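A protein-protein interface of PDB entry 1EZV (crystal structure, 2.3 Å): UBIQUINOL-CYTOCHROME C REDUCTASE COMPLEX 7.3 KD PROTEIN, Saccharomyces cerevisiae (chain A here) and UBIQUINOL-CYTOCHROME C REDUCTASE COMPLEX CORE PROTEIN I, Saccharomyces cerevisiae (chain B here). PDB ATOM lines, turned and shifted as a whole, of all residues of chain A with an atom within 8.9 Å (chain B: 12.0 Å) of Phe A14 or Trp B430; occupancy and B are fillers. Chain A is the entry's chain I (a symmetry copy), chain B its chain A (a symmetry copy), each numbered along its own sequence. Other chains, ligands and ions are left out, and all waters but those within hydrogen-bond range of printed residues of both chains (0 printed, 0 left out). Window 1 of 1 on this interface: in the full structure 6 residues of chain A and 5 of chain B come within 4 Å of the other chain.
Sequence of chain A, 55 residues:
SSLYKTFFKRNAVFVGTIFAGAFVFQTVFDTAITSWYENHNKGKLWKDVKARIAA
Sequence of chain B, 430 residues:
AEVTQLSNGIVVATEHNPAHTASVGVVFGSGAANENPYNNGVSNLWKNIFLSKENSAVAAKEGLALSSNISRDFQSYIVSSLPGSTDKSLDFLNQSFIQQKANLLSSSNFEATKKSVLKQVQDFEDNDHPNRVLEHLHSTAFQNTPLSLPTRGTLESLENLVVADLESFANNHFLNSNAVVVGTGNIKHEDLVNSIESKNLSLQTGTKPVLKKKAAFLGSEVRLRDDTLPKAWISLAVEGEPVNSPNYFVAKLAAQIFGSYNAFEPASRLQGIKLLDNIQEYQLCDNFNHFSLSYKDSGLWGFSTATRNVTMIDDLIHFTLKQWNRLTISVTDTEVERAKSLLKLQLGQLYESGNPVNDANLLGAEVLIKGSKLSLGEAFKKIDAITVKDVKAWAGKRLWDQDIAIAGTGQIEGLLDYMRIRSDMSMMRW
Hydrophobic or aromatic side chains of chain B that line the printed part of chain A: Trp B400 and Trp B430.
Of the 16 printed residues of chain A, 6 touch a printed residue of chain B.
Hydrophobic or aromatic side chains of chain A that line the printed part of chain B: Phe A14, Val A15 and Phe A19.
The backbone NH (N) of Asp B401 is in hydrogen-bond range of the backbone carbonyl oxygen (O) of Met B425 (2.9 Å).
OH of Tyr A4 lies within hydrogen-bond range of O of Asn A11.
The backbone NH (N) of Gly A16 lies within hydrogen-bond range of the chain-end carboxylate (O) of Trp B430 (3.4 Å).
Of chain A, only Phe A14, Val A15, Gly A16 and Phe A19 come within 4 Å of Trp B430.
No residue of chain B comes within 4 Å of Ala A12.
No residue of chain B comes within 4 Å of Val A13.
No residue of chain B comes within 4 Å of Thr A17.
No residue of chain B comes within 4 Å of Ile A18.
Of the printed residues of chain A, Asp B401 touches Arg A10.
Of the printed residues of chain A, Trp B400 touches Asn A11.
Printed residues of chain A within 4 Å of Arg B429: Asn A11 (3.9 Å) and Val A15 (3.4 Å).
Printed residues of chain B within 4 Å of Phe A19: Trp B430 (3.8 Å).
Ser B423 touches none of the printed residues of chain A.
The nearest residue of chain A that does not touch Trp B430 is Thr A17 (5.0 Å).
Asp B401 touches Arg A10.
NE1 of Trp B400 touches ND2 of Asn A11 (3.95 Å).
Asn A11 touches Arg B429 (OD1 to NH1, 3.9 Å).
Phe A14 touches Trp B430.
CG2 of Val A15 touches O of Arg B429, 3.4 Å away.
Val A15 touches Trp B430 (CG2 to CA, 3.96 Å).
CE2 of Phe A19 touches CH2 of Trp B430, at 3.8 Å.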
ATOM      1  N   TYR A   4      32.198 -15.500  -0.387  1.00  0.00           N
ATOM      2  CA  TYR A   4      30.923 -15.029   0.137  1.00  0.00           C
ATOM      3  C   TYR A   4      30.425 -13.802  -0.633  1.00  0.00           C
ATOM      4  O   TYR A   4      29.266 -13.754  -1.050  1.00  0.00           O
ATOM      5  CB  TYR A   4      31.053 -14.699   1.633  1.00  0.00           C
ATOM      6  CG  TYR A   4      29.727 -14.496   2.335  1.00  0.00           C
ATOM      7  CD1 TYR A   4      29.174 -13.221   2.469  1.00  0.00           C
ATOM      8  CD2 TYR A   4      28.982 -15.588   2.787  1.00  0.00           C
ATOM      9  CE1 TYR A   4      27.910 -13.038   3.020  1.00  0.00           C
ATOM     10  CE2 TYR A   4      27.716 -15.414   3.342  1.00  0.00           C
ATOM     11  CZ  TYR A   4      27.188 -14.138   3.450  1.00  0.00           C
ATOM     12  OH  TYR A   4      25.931 -13.960   3.972  1.00  0.00           O
ATOM     13  N   PHE A   7      28.426 -14.389  -4.102  1.00  0.00           N
ATOM     14  CA  PHE A   7      27.055 -14.889  -4.060  1.00  0.00           C
ATOM     15  C   PHE A   7      26.112 -13.936  -3.332  1.00  0.00           C
ATOM     16  O   PHE A   7      25.075 -13.545  -3.870  1.00  0.00           O
ATOM     17  CB  PHE A   7      27.013 -16.256  -3.378  1.00  0.00           C
ATOM     18  CG  PHE A   7      27.740 -17.332  -4.126  1.00  0.00           C
ATOM     19  CD1 PHE A   7      27.166 -17.930  -5.243  1.00  0.00           C
ATOM     20  CD2 PHE A   7      28.986 -17.772  -3.697  1.00  0.00           C
ATOM     21  CE1 PHE A   7      27.822 -18.953  -5.921  1.00  0.00           C
ATOM     22  CE2 PHE A   7      29.651 -18.796  -4.368  1.00  0.00           C
ATOM     23  CZ  PHE A   7      29.068 -19.387  -5.482  1.00  0.00           C
ATOM     24  N   PHE A   8      26.491 -13.550  -2.116  1.00  0.00           N
ATOM     25  CA  PHE A   8      25.585 -12.853  -1.203  1.00  0.00           C
ATOM     26  C   PHE A   8      26.004 -11.408  -0.944  1.00  0.00           C
ATOM     27  O   PHE A   8      25.238 -10.629  -0.373  1.00  0.00           O
ATOM     28  CB  PHE A   8      25.491 -13.621   0.120  1.00  0.00           C
ATOM     29  CG  PHE A   8      25.173 -15.081  -0.052  1.00  0.00           C
ATOM     30  CD1 PHE A   8      23.910 -15.487  -0.476  1.00  0.00           C
ATOM     31  CD2 PHE A   8      26.157 -16.048   0.140  1.00  0.00           C
ATOM     32  CE1 PHE A   8      23.635 -16.833  -0.714  1.00  0.00           C
ATOM     33  CE2 PHE A   8      25.890 -17.397  -0.097  1.00  0.00           C
ATOM     34  CZ  PHE A   8      24.627 -17.787  -0.526  1.00  0.00           C
ATOM     35  N   LYS A   9      27.246 -11.088  -1.303  1.00  0.00           N
ATOM     36  CA  LYS A   9      27.739  -9.710  -1.370  1.00  0.00           C
ATOM     37  C   LYS A   9      27.497  -8.898  -0.101  1.00  0.00           C
ATOM     38  O   LYS A   9      26.649  -8.004  -0.084  1.00  0.00           O
ATOM     39  CB  LYS A   9      27.115  -8.981  -2.566  1.00  0.00           C
ATOM     40  CG  LYS A   9      27.301  -9.683  -3.898  1.00  0.00           C
ATOM     41  CD  LYS A   9      26.523  -8.979  -4.993  1.00  0.00           C
ATOM     42  CE  LYS A   9      26.561  -9.768  -6.291  1.00  0.00           C
ATOM     43  NZ  LYS A   9      25.734  -9.119  -7.348  1.00  0.00           N
ATOM     44  N   ARG A  10      28.232  -9.228   0.958  1.00  0.00           N
ATOM     45  CA  ARG A  10      28.188  -8.499   2.232  1.00  0.00           C
ATOM     46  C   ARG A  10      26.828  -8.491   2.957  1.00  0.00           C
ATOM     47  O   ARG A  10      26.729  -8.056   4.109  1.00  0.00           O
ATOM     48  CB  ARG A  10      28.730  -7.063   2.047  1.00  0.00           C
ATOM     49  CG  ARG A  10      27.697  -5.979   1.750  1.00  0.00           C
ATOM     50  CD  ARG A  10      27.633  -4.948   2.874  1.00  0.00           C
ATOM     51  NE  ARG A  10      28.323  -3.700   2.543  1.00  0.00           N
ATOM     52  CZ  ARG A  10      29.563  -3.393   2.924  1.00  0.00           C
ATOM     53  NH1 ARG A  10      30.078  -2.213   2.608  1.00  0.00           N
ATOM     54  NH2 ARG A  10      30.296  -4.267   3.601  1.00  0.00           N
ATOM     55  N   ASN A  11      25.804  -9.044   2.312  1.00  0.00           N
ATOM     56  CA  ASN A  11      24.507  -9.236   2.949  1.00  0.00           C
ATOM     57  C   ASN A  11      24.393 -10.644   3.513  1.00  0.00           C
ATOM     58  O   ASN A  11      25.035 -11.574   3.020  1.00  0.00           O
ATOM     59  CB  ASN A  11      23.381  -9.000   1.944  1.00  0.00           C
ATOM     60  CG  ASN A  11      22.734  -7.639   2.099  1.00  0.00           C
ATOM     61  OD1 ASN A  11      21.871  -7.264   1.311  1.00  0.00           O
ATOM     62  ND2 ASN A  11      23.148  -6.889   3.114  1.00  0.00           N
ATOM     63  N   ALA A  12      23.574 -10.794   4.550  1.00  0.00           N
ATOM     64  CA  ALA A  12      23.277 -12.112   5.109  1.00  0.00           C
ATOM     65  C   ALA A  12      22.454 -12.949   4.129  1.00  0.00           C
ATOM     66  O   ALA A  12      21.850 -12.415   3.199  1.00  0.00           O
ATOM     67  CB  ALA A  12      22.530 -11.962   6.432  1.00  0.00           C
ATOM     68  N   VAL A  13      22.512 -14.268   4.286  1.00  0.00           N
ATOM     69  CA  VAL A  13      21.687 -15.167   3.489  1.00  0.00           C
ATOM     70  C   VAL A  13      20.234 -15.099   3.962  1.00  0.00           C
ATOM     71  O   VAL A  13      19.962 -15.059   5.164  1.00  0.00           O
ATOM     72  CB  VAL A  13      22.192 -16.617   3.583  1.00  0.00           C
ATOM     73  CG1 VAL A  13      21.464 -17.493   2.571  1.00  0.00           C
ATOM     74  CG2 VAL A  13      23.696 -16.659   3.340  1.00  0.00           C
ATOM     75  N   PHE A  14      19.313 -15.003   3.006  1.00  0.00           N
ATOM     76  CA  PHE A  14      17.901 -14.768   3.303  1.00  0.00           C
ATOM     77  C   PHE A  14      17.136 -16.078   3.457  1.00  0.00           C
ATOM     78  O   PHE A  14      17.459 -17.068   2.793  1.00  0.00           O
ATOM     79  CB  PHE A  14      17.270 -13.923   2.190  1.00  0.00           C
ATOM     80  CG  PHE A  14      17.993 -12.631   1.919  1.00  0.00           C
ATOM     81  CD1 PHE A  14      18.625 -12.417   0.697  1.00  0.00           C
ATOM     82  CD2 PHE A  14      18.060 -11.637   2.892  1.00  0.00           C
ATOM     83  CE1 PHE A  14      19.319 -11.233   0.447  1.00  0.00           C
ATOM     84  CE2 PHE A  14      18.751 -10.448   2.655  1.00  0.00           C
ATOM     85  CZ  PHE A  14      19.382 -10.246   1.430  1.00  0.00           C
ATOM     86  N   VAL A  15      16.075 -16.049   4.269  1.00  0.00           N
ATOM     87  CA  VAL A  15      15.297 -17.249   4.612  1.00  0.00           C
ATOM     88  C   VAL A  15      14.914 -18.112   3.417  1.00  0.00           C
ATOM     89  O   VAL A  15      14.952 -19.338   3.508  1.00  0.00           O
ATOM     90  CB  VAL A  15      13.981 -16.919   5.363  1.00  0.00           C
ATOM     91  CG1 VAL A  15      14.072 -17.395   6.795  1.00  0.00           C
ATOM     92  CG2 VAL A  15      13.672 -15.434   5.299  1.00  0.00           C
ATOM     93  N   GLY A  16      14.480 -17.464   2.331  1.00  0.00           N
ATOM     94  CA  GLY A  16      14.061 -18.178   1.134  1.00  0.00           C
ATOM     95  C   GLY A  16      15.165 -19.041   0.555  1.00  0.00           C
ATOM     96  O   GLY A  16      14.949 -20.215   0.250  1.00  0.00           O
ATOM     97  N   THR A  17      16.372 -18.487   0.507  1.00  0.00           N
ATOM     98  CA  THR A  17      17.559 -19.216   0.064  1.00  0.00           C
ATOM     99  C   THR A  17      17.946 -20.321   1.057  1.00  0.00           C
ATOM    100  O   THR A  17      18.460 -21.373   0.662  1.00  0.00           O
ATOM    101  CB  THR A  17      18.754 -18.257  -0.095  1.00  0.00           C
ATOM    102  OG1 THR A  17      18.350 -17.114  -0.860  1.00  0.00           O
ATOM    103  CG2 THR A  17      19.917 -18.954  -0.791  1.00  0.00           C
ATOM    104  N   ILE A  18      17.759 -20.038   2.347  1.00  0.00           N
ATOM    105  CA  ILE A  18      18.030 -20.994   3.416  1.00  0.00           C
ATOM    106  C   ILE A  18      17.079 -22.184   3.307  1.00  0.00           C
ATOM    107  O   ILE A  18      17.517 -23.332   3.284  1.00  0.00           O
ATOM    108  CB  ILE A  18      17.864 -20.324   4.814  1.00  0.00           C
ATOM    109  CG1 ILE A  18      18.934 -19.247   5.020  1.00  0.00           C
ATOM    110  CG2 ILE A  18      17.931 -21.367   5.918  1.00  0.00           C
ATOM    111  CD1 ILE A  18      20.343 -19.783   5.086  1.00  0.00           C
ATOM    112  N   PHE A  19      15.785 -21.899   3.181  1.00  0.00           N
ATOM    113  CA  PHE A  19      14.768 -22.940   3.066  1.00  0.00           C
ATOM    114  C   PHE A  19      15.018 -23.793   1.829  1.00  0.00           C
ATOM    115  O   PHE A  19      15.025 -25.019   1.909  1.00  0.00           O
ATOM    116  CB  PHE A  19      13.368 -22.318   2.989  1.00  0.00           C
ATOM    117  CG  PHE A  19      12.824 -21.853   4.318  1.00  0.00           C
ATOM    118  CD1 PHE A  19      13.534 -22.064   5.500  1.00  0.00           C
ATOM    119  CD2 PHE A  19      11.578 -21.234   4.391  1.00  0.00           C
ATOM    120  CE1 PHE A  19      13.011 -21.671   6.736  1.00  0.00           C
ATOM    121  CE2 PHE A  19      11.044 -20.839   5.622  1.00  0.00           C
ATOM    122  CZ  PHE A  19      11.764 -21.060   6.798  1.00  0.00           C
ATOM    123  N   ALA A  20      15.339 -23.133   0.720  1.00  0.00           N
ATOM    124  CA  ALA A  20      15.604 -23.813  -0.550  1.00  0.00           C
ATOM    125  C   ALA A  20      16.844 -24.699  -0.470  1.00  0.00           C
ATOM    126  O   ALA A  20      16.833 -25.836  -0.942  1.00  0.00           O
ATOM    127  CB  ALA A  20      15.764 -22.787  -1.672  1.00  0.00           C
ATOM    128  N   GLY A  21      17.904 -24.170   0.136  1.00  0.00           N
ATOM    129  CA  GLY A  21      19.112 -24.946   0.349  1.00  0.00           C
ATOM    130  C   GLY A  21      18.889 -26.157   1.237  1.00  0.00           C
ATOM    131  O   GLY A  21      19.537 -27.188   1.049  1.00  0.00           O
ATOM    132  N   THR B 328      17.081   3.206   2.106  1.00  0.00           N
ATOM    133  CA  THR B 328      17.596   2.191   1.193  1.00  0.00           C
ATOM    134  C   THR B 328      16.464   1.574   0.383  1.00  0.00           C
ATOM    135  O   THR B 328      16.665   1.153  -0.759  1.00  0.00           O
ATOM    136  CB  THR B 328      18.349   1.071   1.950  1.00  0.00           C
ATOM    137  OG1 THR B 328      19.457   1.636   2.654  1.00  0.00           O
ATOM    138  CG2 THR B 328      18.880   0.003   0.987  1.00  0.00           C
ATOM    139  N   ILE B 329      15.260   1.591   0.941  1.00  0.00           N
ATOM    140  CA  ILE B 329      14.193   0.756   0.407  1.00  0.00           C
ATOM    141  C   ILE B 329      12.902   1.467  -0.018  1.00  0.00           C
ATOM    142  O   ILE B 329      12.246   1.022  -0.957  1.00  0.00           O
ATOM    143  CB  ILE B 329      13.835  -0.386   1.394  1.00  0.00           C
ATOM    144  CG1 ILE B 329      13.278   0.194   2.692  1.00  0.00           C
ATOM    145  CG2 ILE B 329      15.066  -1.235   1.693  1.00  0.00           C
ATOM    146  CD1 ILE B 329      12.515  -0.816   3.530  1.00  0.00           C
ATOM    147  N   GLY B 396      22.257   2.506   0.750  1.00  0.00           N
ATOM    148  CA  GLY B 396      22.567   1.090   0.655  1.00  0.00           C
ATOM    149  C   GLY B 396      24.042   0.770   0.819  1.00  0.00           C
ATOM    150  O   GLY B 396      24.422  -0.388   1.012  1.00  0.00           O
ATOM    151  N   TRP B 400      23.026   0.868   5.349  1.00  0.00           N
ATOM    152  CA  TRP B 400      22.430  -0.454   5.476  1.00  0.00           C
ATOM    153  C   TRP B 400      23.426  -1.516   5.939  1.00  0.00           C
ATOM    154  O   TRP B 400      24.318  -1.915   5.181  1.00  0.00           O
ATOM    155  CB  TRP B 400      21.785  -0.882   4.149  1.00  0.00           C
ATOM    156  CG  TRP B 400      20.954  -2.154   4.237  1.00  0.00           C
ATOM    157  CD1 TRP B 400      21.395  -3.438   4.062  1.00  0.00           C
ATOM    158  CD2 TRP B 400      19.549  -2.249   4.513  1.00  0.00           C
ATOM    159  NE1 TRP B 400      20.356  -4.324   4.223  1.00  0.00           N
ATOM    160  CE2 TRP B 400      19.211  -3.623   4.497  1.00  0.00           C
ATOM    161  CE3 TRP B 400      18.542  -1.308   4.770  1.00  0.00           C
ATOM    162  CZ2 TRP B 400      17.910  -4.080   4.727  1.00  0.00           C
ATOM    163  CZ3 TRP B 400      17.242  -1.763   5.003  1.00  0.00           C
ATOM    164  CH2 TRP B 400      16.941  -3.138   4.980  1.00  0.00           C
ATOM    165  N   ASP B 401      23.160  -2.075   7.125  1.00  0.00           N
ATOM    166  CA  ASP B 401      23.987  -3.128   7.714  1.00  0.00           C
ATOM    167  C   ASP B 401      25.448  -2.682   7.821  1.00  0.00           C
ATOM    168  O   ASP B 401      26.368  -3.428   7.507  1.00  0.00           O
ATOM    169  CB  ASP B 401      23.863  -4.413   6.882  1.00  0.00           C
ATOM    170  CG  ASP B 401      24.344  -5.651   7.621  1.00  0.00           C
ATOM    171  OD1 ASP B 401      24.443  -5.632   8.862  1.00  0.00           O
ATOM    172  OD2 ASP B 401      24.587  -6.674   6.948  1.00  0.00           O
ATOM    173  N   SER B 423      22.072  -4.045  15.119  1.00  0.00           N
ATOM    174  CA  SER B 423      21.100  -4.889  14.422  1.00  0.00           C
ATOM    175  C   SER B 423      19.981  -4.079  13.751  1.00  0.00           C
ATOM    176  O   SER B 423      19.422  -4.497  12.738  1.00  0.00           O
ATOM    177  CB  SER B 423      20.489  -5.901  15.398  1.00  0.00           C
ATOM    178  OG  SER B 423      21.470  -6.837  15.817  1.00  0.00           O
ATOM    179  N   MET B 425      20.300  -1.490  12.065  1.00  0.00           N
ATOM    180  CA  MET B 425      20.779  -0.863  10.837  1.00  0.00           C
ATOM    181  C   MET B 425      20.263  -1.582   9.591  1.00  0.00           C
ATOM    182  O   MET B 425      20.741  -1.330   8.483  1.00  0.00           O
ATOM    183  CB  MET B 425      22.311  -0.820  10.807  1.00  0.00           C
ATOM    184  CG  MET B 425      22.925   0.096  11.825  1.00  0.00           C
ATOM    185  SD  MET B 425      22.192   1.738  11.843  1.00  0.00           S
ATOM    186  CE  MET B 425      23.157   2.545  10.572  1.00  0.00           C
ATOM    187  N   SER B 426      19.346  -2.526   9.787  1.00  0.00           N
ATOM    188  CA  SER B 426      18.695  -3.216   8.675  1.00  0.00           C
ATOM    189  C   SER B 426      17.367  -3.841   9.086  1.00  0.00           C
ATOM    190  O   SER B 426      16.871  -3.607  10.192  1.00  0.00           O
ATOM    191  CB  SER B 426      19.612  -4.293   8.094  1.00  0.00           C
ATOM    192  OG  SER B 426      19.916  -5.286   9.051  1.00  0.00           O
ATOM    193  N   MET B 427      16.758  -4.569   8.153  1.00  0.00           N
ATOM    194  CA  MET B 427      15.488  -5.245   8.393  1.00  0.00           C
ATOM    195  C   MET B 427      15.529  -6.668   7.860  1.00  0.00           C
ATOM    196  O   MET B 427      16.197  -6.948   6.861  1.00  0.00           O
ATOM    197  CB  MET B 427      14.345  -4.504   7.703  1.00  0.00           C
ATOM    198  CG  MET B 427      14.122  -3.085   8.168  1.00  0.00           C
ATOM    199  SD  MET B 427      12.819  -2.320   7.200  1.00  0.00           S
ATOM    200  CE  MET B 427      11.397  -2.742   8.204  1.00  0.00           C
ATOM    201  N   MET B 428      14.714  -7.532   8.465  1.00  0.00           N
ATOM    202  CA  MET B 428      14.488  -8.890   7.974  1.00  0.00           C
ATOM    203  C   MET B 428      13.743  -8.857   6.634  1.00  0.00           C
ATOM    204  O   MET B 428      12.813  -8.070   6.454  1.00  0.00           O
ATOM    205  CB  MET B 428      13.662  -9.683   8.995  1.00  0.00           C
ATOM    206  CG  MET B 428      14.304  -9.829  10.377  1.00  0.00           C
ATOM    207  SD  MET B 428      15.694 -10.998  10.413  1.00  0.00           S
ATOM    208  CE  MET B 428      14.835 -12.569  10.320  1.00  0.00           C
ATOM    209  N   ARG B 429      14.175  -9.697   5.695  1.00  0.00           N
ATOM    210  CA  ARG B 429      13.511  -9.837   4.394  1.00  0.00           C
ATOM    211  C   ARG B 429      13.350 -11.314   4.025  1.00  0.00           C
ATOM    212  O   ARG B 429      14.113 -12.166   4.495  1.00  0.00           O
ATOM    213  CB  ARG B 429      14.328  -9.138   3.296  1.00  0.00           C
ATOM    214  CG  ARG B 429      14.518  -7.644   3.499  1.00  0.00           C
ATOM    215  CD  ARG B 429      14.777  -6.936   2.181  1.00  0.00           C
ATOM    216  NE  ARG B 429      16.172  -7.031   1.757  1.00  0.00           N
ATOM    217  CZ  ARG B 429      16.847  -6.037   1.182  1.00  0.00           C
ATOM    218  NH1 ARG B 429      18.116  -6.209   0.832  1.00  0.00           N
ATOM    219  NH2 ARG B 429      16.257  -4.866   0.960  1.00  0.00           N
ATOM    220  N   TRP B 430      12.407 -11.605   3.131  1.00  0.00           N
ATOM    221  CA  TRP B 430      12.307 -12.939   2.539  1.00  0.00           C
ATOM    222  C   TRP B 430      13.366 -13.147   1.446  1.00  0.00           C
ATOM    223  O   TRP B 430      13.941 -14.259   1.390  1.00  0.00           O
ATOM    224  CB  TRP B 430      10.907 -13.176   1.960  1.00  0.00           C
ATOM    225  CG  TRP B 430      10.638 -14.622   1.631  1.00  0.00           C
ATOM    226  CD1 TRP B 430      10.916 -15.268   0.452  1.00  0.00           C
ATOM    227  CD2 TRP B 430      10.139 -15.624   2.525  1.00  0.00           C
ATOM    228  NE1 TRP B 430      10.638 -16.611   0.568  1.00  0.00           N
ATOM    229  CE2 TRP B 430      10.159 -16.858   1.831  1.00  0.00           C
ATOM    230  CE3 TRP B 430       9.684 -15.604   3.853  1.00  0.00           C
ATOM    231  CZ2 TRP B 430       9.748 -18.058   2.419  1.00  0.00           C
ATOM    232  CZ3 TRP B 430       9.274 -16.800   4.438  1.00  0.00           C
ATOM    233  CH2 TRP B 430       9.310 -18.011   3.719  1.00  0.00           C
ATOM    234  OXT TRP B 430      13.624 -12.194   0.676  1.00  0.00           O
